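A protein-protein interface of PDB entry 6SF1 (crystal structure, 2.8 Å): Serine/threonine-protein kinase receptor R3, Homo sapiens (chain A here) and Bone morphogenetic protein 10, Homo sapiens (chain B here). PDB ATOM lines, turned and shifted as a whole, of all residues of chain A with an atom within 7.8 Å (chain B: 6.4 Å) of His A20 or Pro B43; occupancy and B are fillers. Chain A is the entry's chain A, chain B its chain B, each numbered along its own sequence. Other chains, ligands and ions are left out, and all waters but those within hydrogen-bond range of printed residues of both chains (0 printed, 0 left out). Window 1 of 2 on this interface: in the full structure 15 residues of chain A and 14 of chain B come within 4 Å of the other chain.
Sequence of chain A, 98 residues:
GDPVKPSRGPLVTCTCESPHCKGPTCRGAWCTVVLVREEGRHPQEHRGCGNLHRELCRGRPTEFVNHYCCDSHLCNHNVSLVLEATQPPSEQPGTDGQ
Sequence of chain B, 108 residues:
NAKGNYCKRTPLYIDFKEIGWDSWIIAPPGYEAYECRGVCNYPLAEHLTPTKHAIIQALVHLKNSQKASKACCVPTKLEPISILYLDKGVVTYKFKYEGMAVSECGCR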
ATOM      1  N   CYS A  16      26.881   0.030  16.938  1.00  0.00           N
ATOM      2  CA  CYS A  16      26.081   1.040  17.622  1.00  0.00           C
ATOM      3  C   CYS A  16      25.377   0.385  18.806  1.00  0.00           C
ATOM      4  O   CYS A  16      24.493  -0.458  18.623  1.00  0.00           O
ATOM      5  CB  CYS A  16      25.074   1.677  16.667  1.00  0.00           C
ATOM      6  SG  CYS A  16      24.694   3.402  17.047  1.00  0.00           S
ATOM      7  N   GLU A  17      25.778   0.779  20.025  1.00  0.00           N
ATOM      8  CA  GLU A  17      25.163   0.312  21.264  1.00  0.00           C
ATOM      9  C   GLU A  17      25.086   1.502  22.225  1.00  0.00           C
ATOM     10  O   GLU A  17      25.755   1.560  23.256  1.00  0.00           O
ATOM     11  CB  GLU A  17      25.937  -0.860  21.875  1.00  0.00           C
ATOM     12  CG  GLU A  17      25.847  -2.151  21.077  1.00  0.00           C
ATOM     13  CD  GLU A  17      26.618  -3.290  21.716  1.00  0.00           C
ATOM     14  OE1 GLU A  17      27.279  -3.055  22.750  1.00  0.00           O
ATOM     15  OE2 GLU A  17      26.565  -4.417  21.184  1.00  0.00           O
ATOM     16  N   SER A  18      24.255   2.473  21.874  1.00  0.00           N
ATOM     17  CA  SER A  18      24.072   3.692  22.645  1.00  0.00           C
ATOM     18  C   SER A  18      22.602   4.069  22.604  1.00  0.00           C
ATOM     19  O   SER A  18      21.857   3.597  21.737  1.00  0.00           O
ATOM     20  CB  SER A  18      24.930   4.839  22.092  1.00  0.00           C
ATOM     21  OG  SER A  18      24.455   5.271  20.829  1.00  0.00           O
ATOM     22  N   PRO A  19      22.144   4.910  23.538  1.00  0.00           N
ATOM     23  CA  PRO A  19      20.740   5.348  23.501  1.00  0.00           C
ATOM     24  C   PRO A  19      20.356   6.081  22.226  1.00  0.00           C
ATOM     25  O   PRO A  19      19.159   6.175  21.923  1.00  0.00           O
ATOM     26  CB  PRO A  19      20.626   6.265  24.727  1.00  0.00           C
ATOM     27  CG  PRO A  19      21.691   5.785  25.650  1.00  0.00           C
ATOM     28  CD  PRO A  19      22.826   5.354  24.768  1.00  0.00           C
ATOM     29  N   HIS A  20      21.322   6.602  21.467  1.00  0.00           N
ATOM     30  CA  HIS A  20      21.050   7.341  20.241  1.00  0.00           C
ATOM     31  C   HIS A  20      21.254   6.488  18.993  1.00  0.00           C
ATOM     32  O   HIS A  20      21.573   7.018  17.924  1.00  0.00           O
ATOM     33  CB  HIS A  20      21.926   8.591  20.173  1.00  0.00           C
ATOM     34  CG  HIS A  20      22.425   9.051  21.507  1.00  0.00           C
ATOM     35  ND1 HIS A  20      23.746   8.942  21.884  1.00  0.00           N
ATOM     36  CD2 HIS A  20      21.778   9.610  22.557  1.00  0.00           C
ATOM     37  CE1 HIS A  20      23.893   9.420  23.106  1.00  0.00           C
ATOM     38  NE2 HIS A  20      22.714   9.830  23.537  1.00  0.00           N
ATOM     39  N   CYS A  21      21.072   5.175  19.108  1.00  0.00           N
ATOM     40  CA  CYS A  21      21.314   4.248  18.008  1.00  0.00           C
ATOM     41  C   CYS A  21      19.983   3.856  17.381  1.00  0.00           C
ATOM     42  O   CYS A  21      19.163   3.183  18.014  1.00  0.00           O
ATOM     43  CB  CYS A  21      22.072   3.017  18.496  1.00  0.00           C
ATOM     44  SG  CYS A  21      23.806   3.333  18.872  1.00  0.00           S
ATOM     45  N   LYS A  22      19.772   4.278  16.138  1.00  0.00           N
ATOM     46  CA  LYS A  22      18.612   3.853  15.355  1.00  0.00           C
ATOM     47  C   LYS A  22      18.940   2.620  14.519  1.00  0.00           C
ATOM     48  O   LYS A  22      18.700   2.571  13.314  1.00  0.00           O
ATOM     49  CB  LYS A  22      18.124   5.001  14.479  1.00  0.00           C
ATOM     50  CG  LYS A  22      17.619   6.202  15.261  1.00  0.00           C
ATOM     51  CD  LYS A  22      16.951   7.218  14.348  1.00  0.00           C
ATOM     52  CE  LYS A  22      16.353   8.364  15.146  1.00  0.00           C
ATOM     53  NZ  LYS A  22      15.599   9.311  14.280  1.00  0.00           N
ATOM     54  N   GLY A  23      19.504   1.610  15.175  1.00  0.00           N
ATOM     55  CA  GLY A  23      19.930   0.403  14.510  1.00  0.00           C
ATOM     56  C   GLY A  23      21.171  -0.177  15.153  1.00  0.00           C
ATOM     57  O   GLY A  23      21.812   0.451  16.002  1.00  0.00           O
ATOM     58  N   THR A  25      24.056  -0.786  13.713  1.00  0.00           N
ATOM     59  CA  THR A  25      25.273  -0.217  13.154  1.00  0.00           C
ATOM     60  C   THR A  25      25.049   1.251  12.820  1.00  0.00           C
ATOM     61  O   THR A  25      23.922   1.753  12.825  1.00  0.00           O
ATOM     62  CB  THR A  25      25.731  -0.975  11.899  1.00  0.00           C
ATOM     63  OG1 THR A  25      24.696  -0.935  10.909  1.00  0.00           O
ATOM     64  CG2 THR A  25      26.058  -2.423  12.234  1.00  0.00           C
ATOM     65  N   CYS A  26      26.150   1.939  12.526  1.00  0.00           N
ATOM     66  CA  CYS A  26      26.112   3.336  12.126  1.00  0.00           C
ATOM     67  C   CYS A  26      27.328   3.626  11.260  1.00  0.00           C
ATOM     68  O   CYS A  26      28.323   2.898  11.289  1.00  0.00           O
ATOM     69  CB  CYS A  26      26.069   4.272  13.341  1.00  0.00           C
ATOM     70  SG  CYS A  26      27.336   3.938  14.584  1.00  0.00           S
ATOM     71  N   THR A  32      33.594   4.711  17.795  1.00  0.00           N
ATOM     72  CA  THR A  32      33.834   5.184  19.152  1.00  0.00           C
ATOM     73  C   THR A  32      33.369   4.159  20.176  1.00  0.00           C
ATOM     74  O   THR A  32      32.349   3.490  19.986  1.00  0.00           O
ATOM     75  CB  THR A  32      33.115   6.513  19.420  1.00  0.00           C
ATOM     76  OG1 THR A  32      31.698   6.313  19.364  1.00  0.00           O
ATOM     77  CG2 THR A  32      33.513   7.556  18.395  1.00  0.00           C
ATOM     78  N   VAL A  33      34.133   4.045  21.259  1.00  0.00           N
ATOM     79  CA  VAL A  33      33.702   3.388  22.486  1.00  0.00           C
ATOM     80  C   VAL A  33      33.974   4.361  23.623  1.00  0.00           C
ATOM     81  O   VAL A  33      35.131   4.724  23.867  1.00  0.00           O
ATOM     82  CB  VAL A  33      34.427   2.054  22.730  1.00  0.00           C
ATOM     83  CG1 VAL A  33      33.971   1.440  24.044  1.00  0.00           C
ATOM     84  CG2 VAL A  33      34.178   1.095  21.586  1.00  0.00           C
ATOM     85  N   VAL A  34      32.917   4.797  24.301  1.00  0.00           N
ATOM     86  CA  VAL A  34      33.023   5.788  25.366  1.00  0.00           C
ATOM     87  C   VAL A  34      32.543   5.148  26.659  1.00  0.00           C
ATOM     88  O   VAL A  34      31.375   4.753  26.768  1.00  0.00           O
ATOM     89  CB  VAL A  34      32.217   7.057  25.050  1.00  0.00           C
ATOM     90  CG1 VAL A  34      32.583   8.170  26.020  1.00  0.00           C
ATOM     91  CG2 VAL A  34      32.456   7.496  23.612  1.00  0.00           C
ATOM     92  N   LEU A  35      33.441   5.047  27.636  1.00  0.00           N
ATOM     93  CA  LEU A  35      33.118   4.515  28.956  1.00  0.00           C
ATOM     94  C   LEU A  35      32.967   5.691  29.914  1.00  0.00           C
ATOM     95  O   LEU A  35      33.956   6.340  30.272  1.00  0.00           O
ATOM     96  CB  LEU A  35      34.196   3.545  29.434  1.00  0.00           C
ATOM     97  CG  LEU A  35      33.920   2.839  30.761  1.00  0.00           C
ATOM     98  CD1 LEU A  35      32.632   2.033  30.677  1.00  0.00           C
ATOM     99  CD2 LEU A  35      35.088   1.949  31.146  1.00  0.00           C
ATOM    100  N   VAL A  36      31.732   5.961  30.327  1.00  0.00           N
ATOM    101  CA  VAL A  36      31.400   7.110  31.160  1.00  0.00           C
ATOM    102  C   VAL A  36      30.959   6.614  32.527  1.00  0.00           C
ATOM    103  O   VAL A  36      30.239   5.615  32.631  1.00  0.00           O
ATOM    104  CB  VAL A  36      30.296   7.968  30.509  1.00  0.00           C
ATOM    105  CG1 VAL A  36      30.041   9.225  31.323  1.00  0.00           C
ATOM    106  CG2 VAL A  36      30.672   8.316  29.081  1.00  0.00           C
ATOM    107  N   GLN A  44      28.692   3.273  32.410  1.00  0.00           N
ATOM    108  CA  GLN A  44      28.017   2.796  31.211  1.00  0.00           C
ATOM    109  C   GLN A  44      28.975   2.847  30.029  1.00  0.00           C
ATOM    110  O   GLN A  44      29.799   3.763  29.924  1.00  0.00           O
ATOM    111  CB  GLN A  44      26.768   3.629  30.911  1.00  0.00           C
ATOM    112  CG  GLN A  44      25.664   3.485  31.945  1.00  0.00           C
ATOM    113  CD  GLN A  44      24.435   4.306  31.604  1.00  0.00           C
ATOM    114  OE1 GLN A  44      24.432   5.069  30.637  1.00  0.00           O
ATOM    115  NE2 GLN A  44      23.381   4.151  32.398  1.00  0.00           N
ATOM    116  N   GLU A  45      28.862   1.862  29.141  1.00  0.00           N
ATOM    117  CA  GLU A  45      29.760   1.714  28.000  1.00  0.00           C
ATOM    118  C   GLU A  45      28.968   1.975  26.724  1.00  0.00           C
ATOM    119  O   GLU A  45      28.091   1.186  26.357  1.00  0.00           O
ATOM    120  CB  GLU A  45      30.388   0.323  27.987  1.00  0.00           C
ATOM    121  CG  GLU A  45      31.645   0.206  27.145  1.00  0.00           C
ATOM    122  CD  GLU A  45      32.286  -1.165  27.257  1.00  0.00           C
ATOM    123  OE1 GLU A  45      31.543  -2.161  27.372  1.00  0.00           O
ATOM    124  OE2 GLU A  45      33.533  -1.244  27.238  1.00  0.00           O
ATOM    125  N   HIS A  46      29.279   3.079  26.050  1.00  0.00           N
ATOM    126  CA  HIS A  46      28.600   3.472  24.823  1.00  0.00           C
ATOM    127  C   HIS A  46      29.457   3.127  23.613  1.00  0.00           C
ATOM    128  O   HIS A  46      30.675   3.331  23.623  1.00  0.00           O
ATOM    129  CB  HIS A  46      28.290   4.972  24.825  1.00  0.00           C
ATOM    130  CG  HIS A  46      27.376   5.401  25.931  1.00  0.00           C
ATOM    131  ND1 HIS A  46      26.112   5.899  25.699  1.00  0.00           N
ATOM    132  CD2 HIS A  46      27.543   5.411  27.274  1.00  0.00           C
ATOM    133  CE1 HIS A  46      25.539   6.196  26.852  1.00  0.00           C
ATOM    134  NE2 HIS A  46      26.387   5.908  27.823  1.00  0.00           N
ATOM    135  N   ARG A  47      28.814   2.607  22.572  1.00  0.00           N
ATOM    136  CA  ARG A  47      29.479   2.281  21.319  1.00  0.00           C
ATOM    137  C   ARG A  47      28.752   2.963  20.172  1.00  0.00           C
ATOM    138  O   ARG A  47      27.519   2.947  20.109  1.00  0.00           O
ATOM    139  CB  ARG A  47      29.526   0.767  21.081  1.00  0.00           C
ATOM    140  CG  ARG A  47      30.159  -0.022  22.214  1.00  0.00           C
ATOM    141  CD  ARG A  47      30.321  -1.486  21.842  1.00  0.00           C
ATOM    142  NE  ARG A  47      30.708  -2.300  22.991  1.00  0.00           N
ATOM    143  CZ  ARG A  47      31.960  -2.467  23.401  1.00  0.00           C
ATOM    144  NH1 ARG A  47      32.955  -1.875  22.755  1.00  0.00           N
ATOM    145  NH2 ARG A  47      32.219  -3.226  24.458  1.00  0.00           N
ATOM    146  N   LEU A  56      38.283  14.490  21.194  1.00  0.00           N
ATOM    147  CA  LEU A  56      37.814  13.686  22.317  1.00  0.00           C
ATOM    148  C   LEU A  56      38.524  12.342  22.373  1.00  0.00           C
ATOM    149  O   LEU A  56      38.738  11.793  23.459  1.00  0.00           O
ATOM    150  CB  LEU A  56      36.302  13.477  22.227  1.00  0.00           C
ATOM    151  CG  LEU A  56      35.421  14.695  22.503  1.00  0.00           C
ATOM    152  CD1 LEU A  56      33.949  14.333  22.377  1.00  0.00           C
ATOM    153  CD2 LEU A  56      35.721  15.255  23.880  1.00  0.00           C
ATOM    154  N   VAL A  65      35.903   9.107  32.642  1.00  0.00           N
ATOM    155  CA  VAL A  65      35.652   9.019  31.206  1.00  0.00           C
ATOM    156  C   VAL A  65      36.841   8.344  30.536  1.00  0.00           C
ATOM    157  O   VAL A  65      37.988   8.496  30.968  1.00  0.00           O
ATOM    158  CB  VAL A  65      35.365  10.413  30.600  1.00  0.00           C
ATOM    159  CG1 VAL A  65      36.601  11.297  30.652  1.00  0.00           C
ATOM    160  CG2 VAL A  65      34.844  10.286  29.178  1.00  0.00           C
ATOM    161  N   HIS A  67      37.799   7.532  26.309  1.00  0.00           N
ATOM    162  CA  HIS A  67      37.425   7.609  24.902  1.00  0.00           C
ATOM    163  C   HIS A  67      38.326   6.694  24.086  1.00  0.00           C
ATOM    164  O   HIS A  67      39.548   6.886  24.054  1.00  0.00           O
ATOM    165  CB  HIS A  67      37.528   9.042  24.383  1.00  0.00           C
ATOM    166  CG  HIS A  67      36.347   9.896  24.720  1.00  0.00           C
ATOM    167  ND1 HIS A  67      35.271  10.043  23.873  1.00  0.00           N
ATOM    168  CD2 HIS A  67      36.077  10.655  25.809  1.00  0.00           C
ATOM    169  CE1 HIS A  67      34.386  10.853  24.426  1.00  0.00           C
ATOM    170  NE2 HIS A  67      34.851  11.239  25.601  1.00  0.00           N
ATOM    171  N   TYR B   6      16.542  10.854  27.264  1.00  0.00           N
ATOM    172  CA  TYR B   6      17.595  11.677  26.692  1.00  0.00           C
ATOM    173  C   TYR B   6      17.014  12.899  25.983  1.00  0.00           C
ATOM    174  O   TYR B   6      15.815  12.990  25.714  1.00  0.00           O
ATOM    175  CB  TYR B   6      18.455  10.855  25.730  1.00  0.00           C
ATOM    176  CG  TYR B   6      19.874  11.364  25.607  1.00  0.00           C
ATOM    177  CD1 TYR B   6      20.836  11.029  26.553  1.00  0.00           C
ATOM    178  CD2 TYR B   6      20.253  12.182  24.550  1.00  0.00           C
ATOM    179  CE1 TYR B   6      22.134  11.495  26.449  1.00  0.00           C
ATOM    180  CE2 TYR B   6      21.548  12.653  24.440  1.00  0.00           C
ATOM    181  CZ  TYR B   6      22.485  12.306  25.391  1.00  0.00           C
ATOM    182  OH  TYR B   6      23.775  12.771  25.280  1.00  0.00           O
ATOM    183  N   CYS B   7      17.898  13.850  25.687  1.00  0.00           N
ATOM    184  CA  CYS B   7      17.512  15.097  25.038  1.00  0.00           C
ATOM    185  C   CYS B   7      16.940  14.830  23.651  1.00  0.00           C
ATOM    186  O   CYS B   7      17.628  14.297  22.775  1.00  0.00           O
ATOM    187  CB  CYS B   7      18.727  16.019  24.952  1.00  0.00           C
ATOM    188  SG  CYS B   7      18.508  17.548  24.013  1.00  0.00           S
ATOM    189  N   CYS B  40      21.150  15.740  29.011  1.00  0.00           N
ATOM    190  CA  CYS B  40      22.311  15.723  28.123  1.00  0.00           C
ATOM    191  C   CYS B  40      23.467  14.998  28.811  1.00  0.00           C
ATOM    192  O   CYS B  40      24.454  15.596  29.247  1.00  0.00           O
ATOM    193  CB  CYS B  40      22.700  17.145  27.726  1.00  0.00           C
ATOM    194  SG  CYS B  40      21.592  17.942  26.550  1.00  0.00           S
ATOM    195  N   ASN B  41      23.322  13.677  28.909  1.00  0.00           N
ATOM    196  CA  ASN B  41      24.339  12.855  29.546  1.00  0.00           C
ATOM    197  C   ASN B  41      25.507  12.625  28.600  1.00  0.00           C
ATOM    198  O   ASN B  41      25.342  12.542  27.379  1.00  0.00           O
ATOM    199  CB  ASN B  41      23.762  11.509  29.986  1.00  0.00           C
ATOM    200  CG  ASN B  41      22.915  11.616  31.237  1.00  0.00           C
ATOM    201  OD1 ASN B  41      23.117  12.506  32.064  1.00  0.00           O
ATOM    202  ND2 ASN B  41      21.966  10.698  31.387  1.00  0.00           N
ATOM    203  N   TYR B  42      26.692  12.520  29.174  1.00  0.00           N
ATOM    204  CA  TYR B  42      27.891  12.324  28.374  1.00  0.00           C
ATOM    205  C   TYR B  42      28.005  10.860  27.947  1.00  0.00           C
ATOM    206  O   TYR B  42      27.705   9.959  28.735  1.00  0.00           O
ATOM    207  CB  TYR B  42      29.129  12.738  29.164  1.00  0.00           C
ATOM    208  CG  TYR B  42      30.354  12.933  28.309  1.00  0.00           C
ATOM    209  CD1 TYR B  42      30.566  14.125  27.629  1.00  0.00           C
ATOM    210  CD2 TYR B  42      31.294  11.922  28.169  1.00  0.00           C
ATOM    211  CE1 TYR B  42      31.684  14.307  26.838  1.00  0.00           C
ATOM    212  CE2 TYR B  42      32.411  12.095  27.380  1.00  0.00           C
ATOM    213  CZ  TYR B  42      32.604  13.287  26.716  1.00  0.00           C
ATOM    214  OH  TYR B  42      33.721  13.463  25.930  1.00  0.00           O
ATOM    215  N   PRO B  43      28.431  10.588  26.701  1.00  0.00           N
ATOM    216  CA  PRO B  43      28.844  11.563  25.685  1.00  0.00           C
ATOM    217  C   PRO B  43      27.679  12.279  25.006  1.00  0.00           C
ATOM    218  O   PRO B  43      26.632  11.678  24.767  1.00  0.00           O
ATOM    219  CB  PRO B  43      29.604  10.702  24.677  1.00  0.00           C
ATOM    220  CG  PRO B  43      28.954   9.373  24.776  1.00  0.00           C
ATOM    221  CD  PRO B  43      28.580   9.203  26.222  1.00  0.00           C
ATOM    222  N   LEU B  44      27.872  13.561  24.706  1.00  0.00           N
ATOM    223  CA  LEU B  44      26.851  14.338  24.015  1.00  0.00           C
ATOM    224  C   LEU B  44      26.787  13.907  22.553  1.00  0.00           C
ATOM    225  O   LEU B  44      27.763  14.059  21.811  1.00  0.00           O
ATOM    226  CB  LEU B  44      27.154  15.830  24.131  1.00  0.00           C
ATOM    227  CG  LEU B  44      27.361  16.357  25.554  1.00  0.00           C
ATOM    228  CD1 LEU B  44      27.560  17.868  25.557  1.00  0.00           C
ATOM    229  CD2 LEU B  44      26.198  15.962  26.453  1.00  0.00           C
ATOM    230  N   ALA B  45      25.640  13.367  22.147  1.00  0.00           N
ATOM    231  CA  ALA B  45      25.486  12.832  20.801  1.00  0.00           C
ATOM    232  C   ALA B  45      25.657  13.929  19.756  1.00  0.00           C
ATOM    233  O   ALA B  45      25.326  15.096  19.984  1.00  0.00           O
ATOM    234  CB  ALA B  45      24.118  12.168  20.649  1.00  0.00           C
ATOM    235  N   GLU B  46      26.177  13.538  18.589  1.00  0.00           N
ATOM    236  CA  GLU B  46      26.498  14.518  17.556  1.00  0.00           C
ATOM    237  C   GLU B  46      25.249  15.105  16.911  1.00  0.00           C
ATOM    238  O   GLU B  46      25.279  16.251  16.447  1.00  0.00           O
ATOM    239  CB  GLU B  46      27.394  13.886  16.490  1.00  0.00           C
ATOM    240  CG  GLU B  46      28.778  13.520  16.992  1.00  0.00           C
ATOM    241  CD  GLU B  46      29.664  12.962  15.898  1.00  0.00           C
ATOM    242  OE1 GLU B  46      29.138  12.640  14.811  1.00  0.00           O
ATOM    243  OE2 GLU B  46      30.887  12.850  16.124  1.00  0.00           O
ATOM    244  N   HIS B  47      24.147  14.351  16.864  1.00  0.00           N
ATOM    245  CA  HIS B  47      22.929  14.880  16.260  1.00  0.00           C
ATOM    246  C   HIS B  47      22.342  16.028  17.070  1.00  0.00           C
ATOM    247  O   HIS B  47      21.481  16.754  16.561  1.00  0.00           O
ATOM    248  CB  HIS B  47      21.890  13.770  16.085  1.00  0.00           C
ATOM    249  CG  HIS B  47      21.359  13.226  17.374  1.00  0.00           C
ATOM    250  ND1 HIS B  47      20.230  13.728  17.985  1.00  0.00           N
ATOM    251  CD2 HIS B  47      21.801  12.222  18.167  1.00  0.00           C
ATOM    252  CE1 HIS B  47      20.000  13.056  19.100  1.00  0.00           C
ATOM    253  NE2 HIS B  47      20.940  12.139  19.235  1.00  0.00           N
ATOM    254  N   LEU B  48      22.788  16.206  18.312  1.00  0.00           N
ATOM    255  CA  LEU B  48      22.415  17.349  19.130  1.00  0.00           C
ATOM    256  C   LEU B  48      23.407  18.499  19.008  1.00  0.00           C
ATOM    257  O   LEU B  48      23.384  19.414  19.838  1.00  0.00           O
ATOM    258  CB  LEU B  48      22.274  16.920  20.592  1.00  0.00           C
ATOM    259  CG  LEU B  48      21.218  15.840  20.834  1.00  0.00           C
ATOM    260  CD1 LEU B  48      21.210  15.402  22.286  1.00  0.00           C
ATOM    261  CD2 LEU B  48      19.842  16.336  20.414  1.00  0.00           C
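NE2 of His A67 is in hydrogen-bond range of OH of Tyr B42, at 2.5 Å.
The backbone carbonyl oxygen (O) of Val A36 is in hydrogen-bond range of the backbone NH (N) of Gln A44 (2.8 Å). The backbone NH (N) of Val A34 sits at hydrogen-bond distance from the backbone carbonyl oxygen (O) of His A46. OH of Tyr B6 is in hydrogen-bond range of O of Asn B41 (2.6 Å). SG of Cys A16 forms a disulfide with SG of Cys A21 (2.0 Å). The side-chain hydroxyl of Tyr B6 sits at hydrogen-bond distance from the backbone carbonyl oxygen of Pro B43, 3.1 Å away. N of His A20 sits close to OG of Ser A18 (3.5 Å).
Among the printed residues, merely in contact across the chains: His A20 with Tyr B6, His A20 with Pro B43, His A20 with Ala B45, His A20 with His B47, Val A36 with Tyr B42, Val A36 with Pro B43, His A46 with Pro B43, Leu A56 with Tyr B42 and Val A65 with Tyr B42.
Of the printed residues of chain B, Val A65 touches Tyr B42 (3.5 Å). Of the printed residues of chain A, Tyr B42 touches Val A36, Leu A56, Val A65 and His A67. Of the printed residues of chain A, Pro B43 touches His A20 (3.9 Å), Val A36 (3.7 Å) and His A46 (3.999 Å). Of the printed residues of chain A, Ala B45 touches His A20 (3.5 Å). Printed residues of chain A within 4 Å of His B47: His A20. The nearest printed residue of chain B that does not touch His A20 is Leu B44 (5.4 Å). The nearest printed residue of chain A that does not touch Pro B43 is Val A34 (4.01 Å). The nearest printed residue of chain A that does not touch His B47 is Pro A19 (6.8 Å).
Of the 11 printed residues of chain B, 5 touch a printed residue of chain A. Hydrophobic or aromatic side chains of chain B that line the printed part of chain A: Tyr B6, Tyr B42, Pro B43, Ala B45 and His B47. Along chain B the printed residues that touch a printed residue of chain A span positions 6 to 47. Printed residues of chain A that touch a printed residue of chain B: His A20, Val A36, His A46, Leu A56, Val A65 and His A67. Along chain A the printed residues that touch a printed residue of chain B span positions 20 to 67. Among the printed residues, no Asp or Glu carboxylate lies within 4 Å of a Lys or Arg side-chain nitrogen of the other chain.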
